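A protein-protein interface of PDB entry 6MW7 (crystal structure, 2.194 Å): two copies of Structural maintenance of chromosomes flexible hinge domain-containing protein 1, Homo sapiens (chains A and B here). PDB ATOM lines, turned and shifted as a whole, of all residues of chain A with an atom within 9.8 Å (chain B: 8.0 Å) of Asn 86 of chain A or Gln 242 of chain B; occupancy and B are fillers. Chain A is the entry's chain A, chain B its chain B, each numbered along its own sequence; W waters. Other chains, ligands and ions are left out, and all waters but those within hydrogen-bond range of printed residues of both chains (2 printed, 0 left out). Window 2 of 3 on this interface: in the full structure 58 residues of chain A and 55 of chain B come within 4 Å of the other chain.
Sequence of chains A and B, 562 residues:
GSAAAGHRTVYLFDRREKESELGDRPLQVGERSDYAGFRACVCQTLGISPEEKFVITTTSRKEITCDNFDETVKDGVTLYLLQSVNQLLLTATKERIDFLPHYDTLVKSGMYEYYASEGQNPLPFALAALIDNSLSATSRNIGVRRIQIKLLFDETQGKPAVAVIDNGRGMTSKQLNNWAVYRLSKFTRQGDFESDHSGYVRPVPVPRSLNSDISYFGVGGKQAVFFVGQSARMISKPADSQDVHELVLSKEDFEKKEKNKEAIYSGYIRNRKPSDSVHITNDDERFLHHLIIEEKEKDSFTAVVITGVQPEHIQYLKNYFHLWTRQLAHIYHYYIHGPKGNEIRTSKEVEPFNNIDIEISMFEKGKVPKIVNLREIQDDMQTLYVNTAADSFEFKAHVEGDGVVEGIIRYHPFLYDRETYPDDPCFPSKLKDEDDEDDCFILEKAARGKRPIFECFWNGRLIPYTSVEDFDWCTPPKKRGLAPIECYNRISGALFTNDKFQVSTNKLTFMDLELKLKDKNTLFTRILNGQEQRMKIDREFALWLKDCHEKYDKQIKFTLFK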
ATOM      1  N   ARG A  15       0.762 -16.575 -17.634  1.00  0.00           N
ATOM      2  CA  ARG A  15       0.253 -17.439 -18.694  1.00  0.00           C
ATOM      3  C   ARG A  15       0.880 -18.829 -18.626  1.00  0.00           C
ATOM      4  O   ARG A  15       1.136 -19.473 -19.647  1.00  0.00           O
ATOM      5  CB  ARG A  15       0.484 -16.801 -20.066  1.00  0.00           C
ATOM      6  CG  ARG A  15      -0.766 -16.199 -20.691  1.00  0.00           C
ATOM      7  CD  ARG A  15      -1.427 -15.239 -19.727  1.00  0.00           C
ATOM      8  NE  ARG A  15      -2.625 -14.605 -20.261  1.00  0.00           N
ATOM      9  CZ  ARG A  15      -3.539 -14.009 -19.500  1.00  0.00           C
ATOM     10  NH1 ARG A  15      -3.396 -13.979 -18.181  1.00  0.00           N
ATOM     11  NH2 ARG A  15      -4.603 -13.448 -20.050  1.00  0.00           N
ATOM     12  N   ARG A  16       1.118 -19.317 -17.410  1.00  0.00           N
ATOM     13  CA  ARG A  16       1.650 -20.665 -17.250  1.00  0.00           C
ATOM     14  C   ARG A  16       0.591 -21.712 -17.577  1.00  0.00           C
ATOM     15  O   ARG A  16       0.851 -22.662 -18.323  1.00  0.00           O
ATOM     16  CB  ARG A  16       2.180 -20.849 -15.830  1.00  0.00           C
ATOM     17  CG  ARG A  16       3.586 -20.298 -15.625  1.00  0.00           C
ATOM     18  CD  ARG A  16       3.978 -20.330 -14.164  1.00  0.00           C
ATOM     19  NE  ARG A  16       2.990 -19.651 -13.330  1.00  0.00           N
ATOM     20  CZ  ARG A  16       2.774 -19.912 -12.045  1.00  0.00           C
ATOM     21  NH1 ARG A  16       3.472 -20.852 -11.423  1.00  0.00           N
ATOM     22  NH2 ARG A  16       1.850 -19.234 -11.381  1.00  0.00           N
ATOM     23  N   PHE A  54       9.998 -21.754 -14.420  1.00  0.00           N
ATOM     24  CA  PHE A  54       9.268 -20.872 -15.316  1.00  0.00           C
ATOM     25  C   PHE A  54      10.216 -19.851 -15.947  1.00  0.00           C
ATOM     26  O   PHE A  54      11.384 -19.722 -15.567  1.00  0.00           O
ATOM     27  CB  PHE A  54       8.137 -20.163 -14.570  1.00  0.00           C
ATOM     28  CG  PHE A  54       8.608 -19.203 -13.513  1.00  0.00           C
ATOM     29  CD1 PHE A  54       8.955 -17.903 -13.844  1.00  0.00           C
ATOM     30  CD2 PHE A  54       8.694 -19.594 -12.187  1.00  0.00           C
ATOM     31  CE1 PHE A  54       9.389 -17.017 -12.878  1.00  0.00           C
ATOM     32  CE2 PHE A  54       9.126 -18.710 -11.215  1.00  0.00           C
ATOM     33  CZ  PHE A  54       9.473 -17.418 -11.562  1.00  0.00           C
ATOM     34  N   VAL A  55       9.690 -19.118 -16.930  1.00  0.00           N
ATOM     35  CA  VAL A  55      10.454 -18.114 -17.655  1.00  0.00           C
ATOM     36  C   VAL A  55       9.666 -16.812 -17.691  1.00  0.00           C
ATOM     37  O   VAL A  55       8.450 -16.783 -17.483  1.00  0.00           O
ATOM     38  CB  VAL A  55      10.798 -18.564 -19.091  1.00  0.00           C
ATOM     39  CG1 VAL A  55      11.629 -19.833 -19.064  1.00  0.00           C
ATOM     40  CG2 VAL A  55       9.529 -18.766 -19.911  1.00  0.00           C
ATOM     41  N   ILE A  56      10.386 -15.728 -17.965  1.00  0.00           N
ATOM     42  CA  ILE A  56       9.802 -14.411 -18.179  1.00  0.00           C
ATOM     43  C   ILE A  56      10.240 -13.935 -19.554  1.00  0.00           C
ATOM     44  O   ILE A  56      11.436 -13.953 -19.867  1.00  0.00           O
ATOM     45  CB  ILE A  56      10.231 -13.405 -17.093  1.00  0.00           C
ATOM     46  CG1 ILE A  56       9.920 -13.961 -15.703  1.00  0.00           C
ATOM     47  CG2 ILE A  56       9.518 -12.075 -17.299  1.00  0.00           C
ATOM     48  CD1 ILE A  56      10.461 -13.130 -14.561  1.00  0.00           C
ATOM     49  N   THR A  57       9.279 -13.514 -20.372  1.00  0.00           N
ATOM     50  CA  THR A  57       9.560 -13.076 -21.730  1.00  0.00           C
ATOM     51  C   THR A  57       8.822 -11.782 -22.033  1.00  0.00           C
ATOM     52  O   THR A  57       7.808 -11.453 -21.411  1.00  0.00           O
ATOM     53  CB  THR A  57       9.151 -14.128 -22.768  1.00  0.00           C
ATOM     54  OG1 THR A  57       7.720 -14.183 -22.855  1.00  0.00           O
ATOM     55  CG2 THR A  57       9.690 -15.501 -22.394  1.00  0.00           C
ATOM     56  N   THR A  58       9.349 -11.055 -23.015  1.00  0.00           N
ATOM     57  CA  THR A  58       8.629  -9.946 -23.617  1.00  0.00           C
ATOM     58  C   THR A  58       7.474 -10.491 -24.458  1.00  0.00           C
ATOM     59  O   THR A  58       7.294 -11.702 -24.610  1.00  0.00           O
ATOM     60  CB  THR A  58       9.577  -9.103 -24.466  1.00  0.00           C
ATOM     61  OG1 THR A  58      10.044  -9.879 -25.579  1.00  0.00           O
ATOM     62  CG2 THR A  58      10.777  -8.644 -23.635  1.00  0.00           C
ATOM     63  N   THR A  59       6.678  -9.582 -25.022  1.00  0.00           N
ATOM     64  CA  THR A  59       5.587 -10.012 -25.887  1.00  0.00           C
ATOM     65  C   THR A  59       6.083 -10.621 -27.193  1.00  0.00           C
ATOM     66  O   THR A  59       5.280 -11.206 -27.929  1.00  0.00           O
ATOM     67  CB  THR A  59       4.647  -8.840 -26.169  1.00  0.00           C
ATOM     68  OG1 THR A  59       5.390  -7.742 -26.712  1.00  0.00           O
ATOM     69  CG2 THR A  59       3.957  -8.415 -24.877  1.00  0.00           C
ATOM     70  N   SER A  60       7.373 -10.499 -27.499  1.00  0.00           N
ATOM     71  CA  SER A  60       7.962 -11.164 -28.652  1.00  0.00           C
ATOM     72  C   SER A  60       8.590 -12.507 -28.301  1.00  0.00           C
ATOM     73  O   SER A  60       9.231 -13.117 -29.163  1.00  0.00           O
ATOM     74  CB  SER A  60       9.019 -10.263 -29.296  1.00  0.00           C
ATOM     75  OG  SER A  60      10.120 -10.071 -28.425  1.00  0.00           O
ATOM     76  N   ARG A  61       8.427 -12.973 -27.062  1.00  0.00           N
ATOM     77  CA  ARG A  61       9.011 -14.230 -26.589  1.00  0.00           C
ATOM     78  C   ARG A  61      10.526 -14.135 -26.419  1.00  0.00           C
ATOM     79  O   ARG A  61      11.227 -15.147 -26.485  1.00  0.00           O
ATOM     80  CB  ARG A  61       8.658 -15.415 -27.499  1.00  0.00           C
ATOM     81  CG  ARG A  61       7.163 -15.631 -27.699  1.00  0.00           C
ATOM     82  CD  ARG A  61       6.465 -15.932 -26.384  1.00  0.00           C
ATOM     83  NE  ARG A  61       5.033 -16.164 -26.560  1.00  0.00           N
ATOM     84  CZ  ARG A  61       4.417 -17.335 -26.416  1.00  0.00           C
ATOM     85  NH1 ARG A  61       5.086 -18.427 -26.078  1.00  0.00           N
ATOM     86  NH2 ARG A  61       3.106 -17.411 -26.605  1.00  0.00           N
ATOM     87  N   LYS A  62      11.047 -12.932 -26.187  1.00  0.00           N
ATOM     88  CA  LYS A  62      12.446 -12.771 -25.814  1.00  0.00           C
ATOM     89  C   LYS A  62      12.574 -12.948 -24.306  1.00  0.00           C
ATOM     90  O   LYS A  62      11.974 -12.193 -23.534  1.00  0.00           O
ATOM     91  CB  LYS A  62      12.970 -11.402 -26.244  1.00  0.00           C
ATOM     92  CG  LYS A  62      14.389 -11.118 -25.770  1.00  0.00           C
ATOM     93  CD  LYS A  62      14.973  -9.867 -26.408  1.00  0.00           C
ATOM     94  CE  LYS A  62      16.336  -9.536 -25.813  1.00  0.00           C
ATOM     95  NZ  LYS A  62      16.909  -8.275 -26.360  1.00  0.00           N
ATOM     96  N   GLU A  63      13.355 -13.942 -23.886  1.00  0.00           N
ATOM     97  CA  GLU A  63      13.436 -14.290 -22.474  1.00  0.00           C
ATOM     98  C   GLU A  63      14.265 -13.263 -21.714  1.00  0.00           C
ATOM     99  O   GLU A  63      15.339 -12.857 -22.168  1.00  0.00           O
ATOM    100  CB  GLU A  63      14.039 -15.683 -22.294  1.00  0.00           C
ATOM    101  CG  GLU A  63      13.922 -16.209 -20.871  1.00  0.00           C
ATOM    102  CD  GLU A  63      14.452 -17.619 -20.719  1.00  0.00           C
ATOM    103  OE1 GLU A  63      15.101 -18.119 -21.662  1.00  0.00           O
ATOM    104  OE2 GLU A  63      14.217 -18.232 -19.655  1.00  0.00           O
ATOM    105  N   TYR A  80       5.495 -11.677 -19.851  1.00  0.00           N
ATOM    106  CA  TYR A  80       4.782 -12.942 -19.746  1.00  0.00           C
ATOM    107  C   TYR A  80       5.471 -13.860 -18.744  1.00  0.00           C
ATOM    108  O   TYR A  80       6.698 -13.981 -18.743  1.00  0.00           O
ATOM    109  CB  TYR A  80       4.715 -13.662 -21.105  1.00  0.00           C
ATOM    110  CG  TYR A  80       3.860 -12.995 -22.163  1.00  0.00           C
ATOM    111  CD1 TYR A  80       2.916 -12.035 -21.828  1.00  0.00           C
ATOM    112  CD2 TYR A  80       3.993 -13.341 -23.503  1.00  0.00           C
ATOM    113  CE1 TYR A  80       2.136 -11.432 -22.798  1.00  0.00           C
ATOM    114  CE2 TYR A  80       3.218 -12.746 -24.478  1.00  0.00           C
ATOM    115  CZ  TYR A  80       2.290 -11.793 -24.122  1.00  0.00           C
ATOM    116  OH  TYR A  80       1.517 -11.201 -25.095  1.00  0.00           O
ATOM    117  N   LEU A  81       4.673 -14.507 -17.900  1.00  0.00           N
ATOM    118  CA  LEU A  81       5.117 -15.654 -17.116  1.00  0.00           C
ATOM    119  C   LEU A  81       4.707 -16.919 -17.855  1.00  0.00           C
ATOM    120  O   LEU A  81       3.512 -17.179 -18.023  1.00  0.00           O
ATOM    121  CB  LEU A  81       4.500 -15.657 -15.717  1.00  0.00           C
ATOM    122  CG  LEU A  81       5.122 -14.925 -14.528  1.00  0.00           C
ATOM    123  CD1 LEU A  81       4.666 -15.604 -13.240  1.00  0.00           C
ATOM    124  CD2 LEU A  81       6.630 -14.863 -14.599  1.00  0.00           C
ATOM    125  N   LEU A  82       5.690 -17.709 -18.273  1.00  0.00           N
ATOM    126  CA  LEU A  82       5.437 -18.905 -19.059  1.00  0.00           C
ATOM    127  C   LEU A  82       6.182 -20.089 -18.465  1.00  0.00           C
ATOM    128  O   LEU A  82       7.222 -19.932 -17.819  1.00  0.00           O
ATOM    129  CB  LEU A  82       5.861 -18.703 -20.519  1.00  0.00           C
ATOM    130  CG  LEU A  82       5.261 -17.475 -21.204  1.00  0.00           C
ATOM    131  CD1 LEU A  82       5.975 -17.187 -22.512  1.00  0.00           C
ATOM    132  CD2 LEU A  82       3.772 -17.672 -21.431  1.00  0.00           C
ATOM    133  N   GLN A  83       5.628 -21.285 -18.682  1.00  0.00           N
ATOM    134  CA  GLN A  83       6.352 -22.502 -18.339  1.00  0.00           C
ATOM    135  C   GLN A  83       7.614 -22.640 -19.176  1.00  0.00           C
ATOM    136  O   GLN A  83       8.624 -23.171 -18.700  1.00  0.00           O
ATOM    137  CB  GLN A  83       5.461 -23.729 -18.538  1.00  0.00           C
ATOM    138  CG  GLN A  83       4.188 -23.729 -17.710  1.00  0.00           C
ATOM    139  CD  GLN A  83       3.415 -25.026 -17.847  1.00  0.00           C
ATOM    140  OE1 GLN A  83       3.779 -25.897 -18.637  1.00  0.00           O
ATOM    141  NE2 GLN A  83       2.342 -25.163 -17.075  1.00  0.00           N
ATOM    142  N   SER A  84       7.575 -22.170 -20.420  1.00  0.00           N
ATOM    143  CA  SER A  84       8.730 -22.215 -21.300  1.00  0.00           C
ATOM    144  C   SER A  84       8.622 -21.073 -22.301  1.00  0.00           C
ATOM    145  O   SER A  84       7.556 -20.478 -22.482  1.00  0.00           O
ATOM    146  CB  SER A  84       8.836 -23.567 -22.018  1.00  0.00           C
ATOM    147  OG  SER A  84       7.804 -23.717 -22.976  1.00  0.00           O
ATOM    148  N   VAL A  85       9.746 -20.781 -22.956  1.00  0.00           N
ATOM    149  CA  VAL A  85       9.839 -19.588 -23.794  1.00  0.00           C
ATOM    150  C   VAL A  85       8.788 -19.611 -24.899  1.00  0.00           C
ATOM    151  O   VAL A  85       8.219 -18.571 -25.254  1.00  0.00           O
ATOM    152  CB  VAL A  85      11.264 -19.456 -24.363  1.00  0.00           C
ATOM    153  CG1 VAL A  85      11.302 -18.532 -25.582  1.00  0.00           C
ATOM    154  CG2 VAL A  85      12.205 -18.935 -23.286  1.00  0.00           C
ATOM    155  N   ASN A  86       8.513 -20.788 -25.462  1.00  0.00           N
ATOM    156  CA  ASN A  86       7.633 -20.908 -26.620  1.00  0.00           C
ATOM    157  C   ASN A  86       6.358 -21.676 -26.289  1.00  0.00           C
ATOM    158  O   ASN A  86       5.762 -22.308 -27.163  1.00  0.00           O
ATOM    159  CB  ASN A  86       8.370 -21.566 -27.785  1.00  0.00           C
ATOM    160  CG  ASN A  86       9.474 -20.688 -28.344  1.00  0.00           C
ATOM    161  OD1 ASN A  86      10.628 -21.107 -28.439  1.00  0.00           O
ATOM    162  ND2 ASN A  86       9.124 -19.462 -28.716  1.00  0.00           N
ATOM    163  N   GLN A  87       5.925 -21.626 -25.032  1.00  0.00           N
ATOM    164  CA  GLN A  87       4.650 -22.217 -24.659  1.00  0.00           C
ATOM    165  C   GLN A  87       3.534 -21.646 -25.525  1.00  0.00           C
ATOM    166  O   GLN A  87       3.614 -20.514 -26.012  1.00  0.00           O
ATOM    167  CB  GLN A  87       4.354 -21.953 -23.181  1.00  0.00           C
ATOM    168  CG  GLN A  87       3.061 -22.579 -22.672  1.00  0.00           C
ATOM    169  CD  GLN A  87       2.721 -22.140 -21.265  1.00  0.00           C
ATOM    170  OE1 GLN A  87       3.553 -21.564 -20.563  1.00  0.00           O
ATOM    171  NE2 GLN A  87       1.489 -22.399 -20.847  1.00  0.00           N
ATOM    172  N   LEU A  88       2.487 -22.442 -25.723  1.00  0.00           N
ATOM    173  CA  LEU A  88       1.326 -21.978 -26.469  1.00  0.00           C
ATOM    174  C   LEU A  88       0.549 -20.969 -25.635  1.00  0.00           C
ATOM    175  O   LEU A  88       0.283 -21.201 -24.451  1.00  0.00           O
ATOM    176  CB  LEU A  88       0.431 -23.159 -26.843  1.00  0.00           C
ATOM    177  CG  LEU A  88      -0.483 -22.966 -28.054  1.00  0.00           C
ATOM    178  CD1 LEU A  88       0.328 -22.939 -29.342  1.00  0.00           C
ATOM    179  CD2 LEU A  88      -1.537 -24.060 -28.103  1.00  0.00           C
ATOM    180  N   LEU A  89       0.189 -19.845 -26.248  1.00  0.00           N
ATOM    181  CA  LEU A  89      -0.566 -18.807 -25.553  1.00  0.00           C
ATOM    182  C   LEU A  89      -2.013 -19.272 -25.442  1.00  0.00           C
ATOM    183  O   LEU A  89      -2.811 -19.103 -26.367  1.00  0.00           O
ATOM    184  CB  LEU A  89      -0.451 -17.476 -26.290  1.00  0.00           C
ATOM    185  CG  LEU A  89      -0.898 -16.202 -25.566  1.00  0.00           C
ATOM    186  CD1 LEU A  89      -0.352 -16.123 -24.147  1.00  0.00           C
ATOM    187  CD2 LEU A  89      -0.448 -14.986 -26.364  1.00  0.00           C
ATOM    188  N   LEU A  90      -2.353 -19.866 -24.297  1.00  0.00           N
ATOM    189  CA  LEU A  90      -3.669 -20.469 -24.113  1.00  0.00           C
ATOM    190  C   LEU A  90      -4.758 -19.421 -23.927  1.00  0.00           C
ATOM    191  O   LEU A  90      -5.914 -19.664 -24.288  1.00  0.00           O
ATOM    192  CB  LEU A  90      -3.640 -21.411 -22.909  1.00  0.00           C
ATOM    193  CG  LEU A  90      -2.474 -22.406 -22.887  1.00  0.00           C
ATOM    194  CD1 LEU A  90      -2.365 -23.084 -21.533  1.00  0.00           C
ATOM    195  CD2 LEU A  90      -2.624 -23.437 -23.994  1.00  0.00           C
ATOM    196  N   LYS B 237       1.183 -10.941 -38.024  1.00  0.00           N
ATOM    197  CA  LYS B 237       2.021 -11.964 -37.416  1.00  0.00           C
ATOM    198  C   LYS B 237       3.298 -12.135 -38.229  1.00  0.00           C
ATOM    199  O   LYS B 237       3.237 -12.605 -39.371  1.00  0.00           O
ATOM    200  CB  LYS B 237       1.272 -13.293 -37.333  1.00  0.00           C
ATOM    201  CG  LYS B 237       2.103 -14.455 -36.782  1.00  0.00           C
ATOM    202  CD  LYS B 237       1.511 -15.800 -37.169  1.00  0.00           C
ATOM    203  CE  LYS B 237       2.411 -16.956 -36.748  1.00  0.00           C
ATOM    204  NZ  LYS B 237       3.782 -16.864 -37.336  1.00  0.00           N
ATOM    205  N   PRO B 238       4.462 -11.769 -37.700  1.00  0.00           N
ATOM    206  CA  PRO B 238       5.711 -12.107 -38.390  1.00  0.00           C
ATOM    207  C   PRO B 238       5.948 -13.608 -38.377  1.00  0.00           C
ATOM    208  O   PRO B 238       5.372 -14.351 -37.579  1.00  0.00           O
ATOM    209  CB  PRO B 238       6.789 -11.368 -37.587  1.00  0.00           C
ATOM    210  CG  PRO B 238       6.058 -10.390 -36.726  1.00  0.00           C
ATOM    211  CD  PRO B 238       4.694 -10.950 -36.501  1.00  0.00           C
ATOM    212  N   ALA B 239       6.815 -14.055 -39.287  1.00  0.00           N
ATOM    213  CA  ALA B 239       7.160 -15.471 -39.327  1.00  0.00           C
ATOM    214  C   ALA B 239       7.929 -15.881 -38.079  1.00  0.00           C
ATOM    215  O   ALA B 239       7.765 -17.000 -37.579  1.00  0.00           O
ATOM    216  CB  ALA B 239       7.977 -15.783 -40.579  1.00  0.00           C
ATOM    217  N   ASP B 240       8.769 -14.986 -37.562  1.00  0.00           N
ATOM    218  CA  ASP B 240       9.535 -15.233 -36.348  1.00  0.00           C
ATOM    219  C   ASP B 240       8.723 -14.997 -35.070  1.00  0.00           C
ATOM    220  O   ASP B 240       9.320 -14.803 -34.005  1.00  0.00           O
ATOM    221  CB  ASP B 240      10.790 -14.354 -36.331  1.00  0.00           C
ATOM    222  N   SER B 241       7.394 -15.007 -35.146  1.00  0.00           N
ATOM    223  CA  SER B 241       6.538 -14.754 -33.995  1.00  0.00           C
ATOM    224  C   SER B 241       5.537 -15.889 -33.852  1.00  0.00           C
ATOM    225  O   SER B 241       4.895 -16.284 -34.830  1.00  0.00           O
ATOM    226  CB  SER B 241       5.800 -13.420 -34.139  1.00  0.00           C
ATOM    227  OG  SER B 241       4.796 -13.263 -33.148  1.00  0.00           O
ATOM    228  N   GLN B 242       5.412 -16.407 -32.631  1.00  0.00           N
ATOM    229  CA  GLN B 242       4.454 -17.461 -32.331  1.00  0.00           C
ATOM    230  C   GLN B 242       3.062 -16.917 -32.032  1.00  0.00           C
ATOM    231  O   GLN B 242       2.082 -17.660 -32.156  1.00  0.00           O
ATOM    232  CB  GLN B 242       4.982 -18.281 -31.153  1.00  0.00           C
ATOM    233  CG  GLN B 242       3.980 -19.191 -30.476  1.00  0.00           C
ATOM    234  CD  GLN B 242       4.618 -19.979 -29.350  1.00  0.00           C
ATOM    235  OE1 GLN B 242       5.827 -19.898 -29.134  1.00  0.00           O
ATOM    236  NE2 GLN B 242       3.810 -20.738 -28.621  1.00  0.00           N
ATOM    237  N   ASP B 243       2.954 -15.647 -31.651  1.00  0.00           N
ATOM    238  CA  ASP B 243       1.678 -15.012 -31.359  1.00  0.00           C
ATOM    239  C   ASP B 243       1.261 -14.087 -32.497  1.00  0.00           C
ATOM    240  O   ASP B 243       2.087 -13.590 -33.265  1.00  0.00           O
ATOM    241  CB  ASP B 243       1.758 -14.215 -30.056  1.00  0.00           C
ATOM    242  CG  ASP B 243       2.092 -15.083 -28.864  1.00  0.00           C
ATOM    243  OD1 ASP B 243       1.626 -16.241 -28.825  1.00  0.00           O
ATOM    244  OD2 ASP B 243       2.819 -14.609 -27.966  1.00  0.00           O
ATOM    245  N   VAL B 244      -0.048 -13.866 -32.594  1.00  0.00           N
ATOM    246  CA  VAL B 244      -0.628 -12.916 -33.538  1.00  0.00           C
ATOM    247  C   VAL B 244      -0.949 -11.635 -32.781  1.00  0.00           C
ATOM    248  O   VAL B 244      -1.393 -11.681 -31.626  1.00  0.00           O
ATOM    249  CB  VAL B 244      -1.885 -13.505 -34.208  1.00  0.00           C
ATOM    250  CG1 VAL B 244      -2.602 -12.462 -35.053  1.00  0.00           C
ATOM    251  CG2 VAL B 244      -1.515 -14.713 -35.064  1.00  0.00           C
ATOM    252  N   HIS B 245      -0.725 -10.490 -33.425  1.00  0.00           N
ATOM    253  CA  HIS B 245      -0.910  -9.181 -32.805  1.00  0.00           C
ATOM    254  C   HIS B 245      -2.083  -8.463 -33.462  1.00  0.00           C
ATOM    255  O   HIS B 245      -2.155  -8.378 -34.692  1.00  0.00           O
ATOM    256  CB  HIS B 245       0.362  -8.342 -32.925  1.00  0.00           C
ATOM    257  CG  HIS B 245       1.612  -9.088 -32.575  1.00  0.00           C
ATOM    258  ND1 HIS B 245       1.846  -9.604 -31.319  1.00  0.00           N
ATOM    259  CD2 HIS B 245       2.699  -9.403 -33.319  1.00  0.00           C
ATOM    260  CE1 HIS B 245       3.023 -10.205 -31.304  1.00  0.00           C
ATOM    261  NE2 HIS B 245       3.560 -10.098 -32.505  1.00  0.00           N
ATOM    262  N   ARG B 272      -2.414 -13.163 -29.231  1.00  0.00           N
ATOM    263  CA  ARG B 272      -3.187 -14.392 -29.156  1.00  0.00           C
ATOM    264  C   ARG B 272      -2.537 -15.431 -30.052  1.00  0.00           C
ATOM    265  O   ARG B 272      -1.697 -15.107 -30.895  1.00  0.00           O
ATOM    266  CB  ARG B 272      -4.643 -14.159 -29.569  1.00  0.00           C
ATOM    267  CG  ARG B 272      -4.815 -13.645 -30.999  1.00  0.00           C
ATOM    268  CD  ARG B 272      -6.281 -13.631 -31.412  1.00  0.00           C
ATOM    269  NE  ARG B 272      -6.491 -12.961 -32.692  1.00  0.00           N
ATOM    270  CZ  ARG B 272      -6.148 -13.468 -33.873  1.00  0.00           C
ATOM    271  NH1 ARG B 272      -5.562 -14.654 -33.952  1.00  0.00           N
ATOM    272  NH2 ARG B 272      -6.385 -12.781 -34.981  1.00  0.00           N
ATOM    273  N   LYS B 273      -2.934 -16.682 -29.859  1.00  0.00           N
ATOM    274  CA  LYS B 273      -2.448 -17.724 -30.746  1.00  0.00           C
ATOM    275  C   LYS B 273      -3.175 -17.649 -32.089  1.00  0.00           C
ATOM    276  O   LYS B 273      -4.314 -17.180 -32.160  1.00  0.00           O
ATOM    277  CB  LYS B 273      -2.656 -19.102 -30.124  1.00  0.00           C
ATOM    278  CG  LYS B 273      -4.106 -19.425 -29.785  1.00  0.00           C
ATOM    279  CD  LYS B 273      -4.288 -20.888 -29.404  1.00  0.00           C
ATOM    280  CE  LYS B 273      -5.713 -21.157 -28.944  1.00  0.00           C
ATOM    281  NZ  LYS B 273      -6.026 -22.609 -28.825  1.00  0.00           N
ATOM    282  N   PRO B 274      -2.535 -18.090 -33.172  1.00  0.00           N
ATOM    283  CA  PRO B 274      -3.221 -18.123 -34.470  1.00  0.00           C
ATOM    284  C   PRO B 274      -4.559 -18.845 -34.395  1.00  0.00           C
ATOM    285  O   PRO B 274      -4.711 -19.842 -33.688  1.00  0.00           O
ATOM    286  CB  PRO B 274      -2.230 -18.870 -35.367  1.00  0.00           C
ATOM    287  CG  PRO B 274      -0.897 -18.570 -34.784  1.00  0.00           C
ATOM    288  CD  PRO B 274      -1.102 -18.414 -33.297  1.00  0.00           C
ATOM    289  N   ASP B 299       2.466 -18.618 -42.300  1.00  0.00           N
ATOM    290  CA  ASP B 299       3.572 -18.318 -41.397  1.00  0.00           C
ATOM    291  C   ASP B 299       3.627 -16.830 -41.071  1.00  0.00           C
ATOM    292  O   ASP B 299       3.873 -16.451 -39.920  1.00  0.00           O
ATOM    293  CB  ASP B 299       4.891 -18.780 -42.015  1.00  0.00           C
ATOM    294  CG  ASP B 299       4.924 -20.274 -42.270  1.00  0.00           C
ATOM    295  OD1 ASP B 299       4.335 -21.027 -41.468  1.00  0.00           O
ATOM    296  OD2 ASP B 299       5.537 -20.693 -43.275  1.00  0.00           O
HETATM  297  O   HOH W   1       0.610 -18.867 -29.236  1.00  0.00           O
HETATM  298  O   HOH W   2       2.860 -11.663 -27.407  1.00  0.00           O
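Water W1 lies within hydrogen-bond range of OD1 of Asp 243 of chain B (2.8 Å), N of Leu 89 of chain A (3.2 Å) and O of Gln 242 of chain B (3.5 Å).
Of chain B, only Gln 242 (2.9 Å) comes within 4 Å of Asn 86 of chain A.
Gln 242 of chain B touches four residues of chain A.
Asp 243 of chain B touches just these residues of chain A: Arg 61 (2.9 Å), Tyr 80 (3.97 Å) and Leu 89 (3.5 Å).
Of the printed residues of chain A, Arg 272 of chain B touches Leu 89.
Printed residues of chain B within 4 Å of Leu 89 of chain A: Asp 243 (3.5 Å), Arg 272 (3.9 Å) and Lys 273 (3.7 Å).
Ser 84 of chain A touches none of the printed residues of chain B.
Thr 58 of chain A touches none of the printed residues of chain B.
The nearest residue of chain B that does not touch Asn 86 of chain A is Asp 240 of chain B (7.1 Å).
The nearest residue of chain A that does not touch Gln 242 of chain B is Leu 89 of chain A (4.4 Å).
The nearest printed residue of chain A that does not touch Arg 272 of chain B is Tyr 80 of chain A (6.0 Å).
Hydrophobic or aromatic side chains of chain A within 4 Å of the printed part of chain B: Tyr 80 and Leu 89.
Among the printed residues, 9 pairs touch across the chains.
Among the printed residues, Asp or Glu carboxylates within 4 Å of a Lys or Arg side-chain nitrogen of the other chain: Arg 61 of chain A with Asp 243 of chain B.
The guanidinium group (NH1) of Arg 61 of chain A lies within hydrogen-bond range of the backbone carbonyl oxygen (O) of Gln 87 of chain A, 2.6 Å away.
The backbone NH (N) of Gln 83 of chain A sits at hydrogen-bond distance from the side-chain amide oxygen (OE1) of Gln 87 of chain A.
Tyr 80 of chain A touches Asp 243 of chain B (CE2 to OD2, 3.97 Å).
NE2 of Gln 242 of chain B touches CA of Leu 88 of chain A, at 3.5 Å.
Leu 89 of chain A touches Asp 243 of chain B (CD2 to OD1, 3.5 Å).
Leu 89 of chain A touches Arg 272 of chain B (CD2 to N, 3.9 Å).
O of Leu 89 of chain A touches CG of Lys 273 of chain B (3.7 Å).
The guanidinium group (NH2) of Arg 61 of chain A lies within salt-bridge range of the side-chain carboxylate (OD1) of Asp 243 of chain B (2.9 Å).
The guanidinium group (NH1) of Arg 61 of chain A is in hydrogen-bond range of the side-chain amide oxygen (OE1) of Gln 242 of chain B (3.5 Å).
O of Asn 86 of chain A sits at hydrogen-bond distance from NE2 of Gln 242 of chain B.
O of Gln 87 of chain A sits at hydrogen-bond distance from NE2 of Gln 242 of chain B, 2.6 Å away.
No position is printed for both chains.
Of the 9 pairs that touch across the chains among the printed residues, none has its exchanged pair printed and touching as well.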
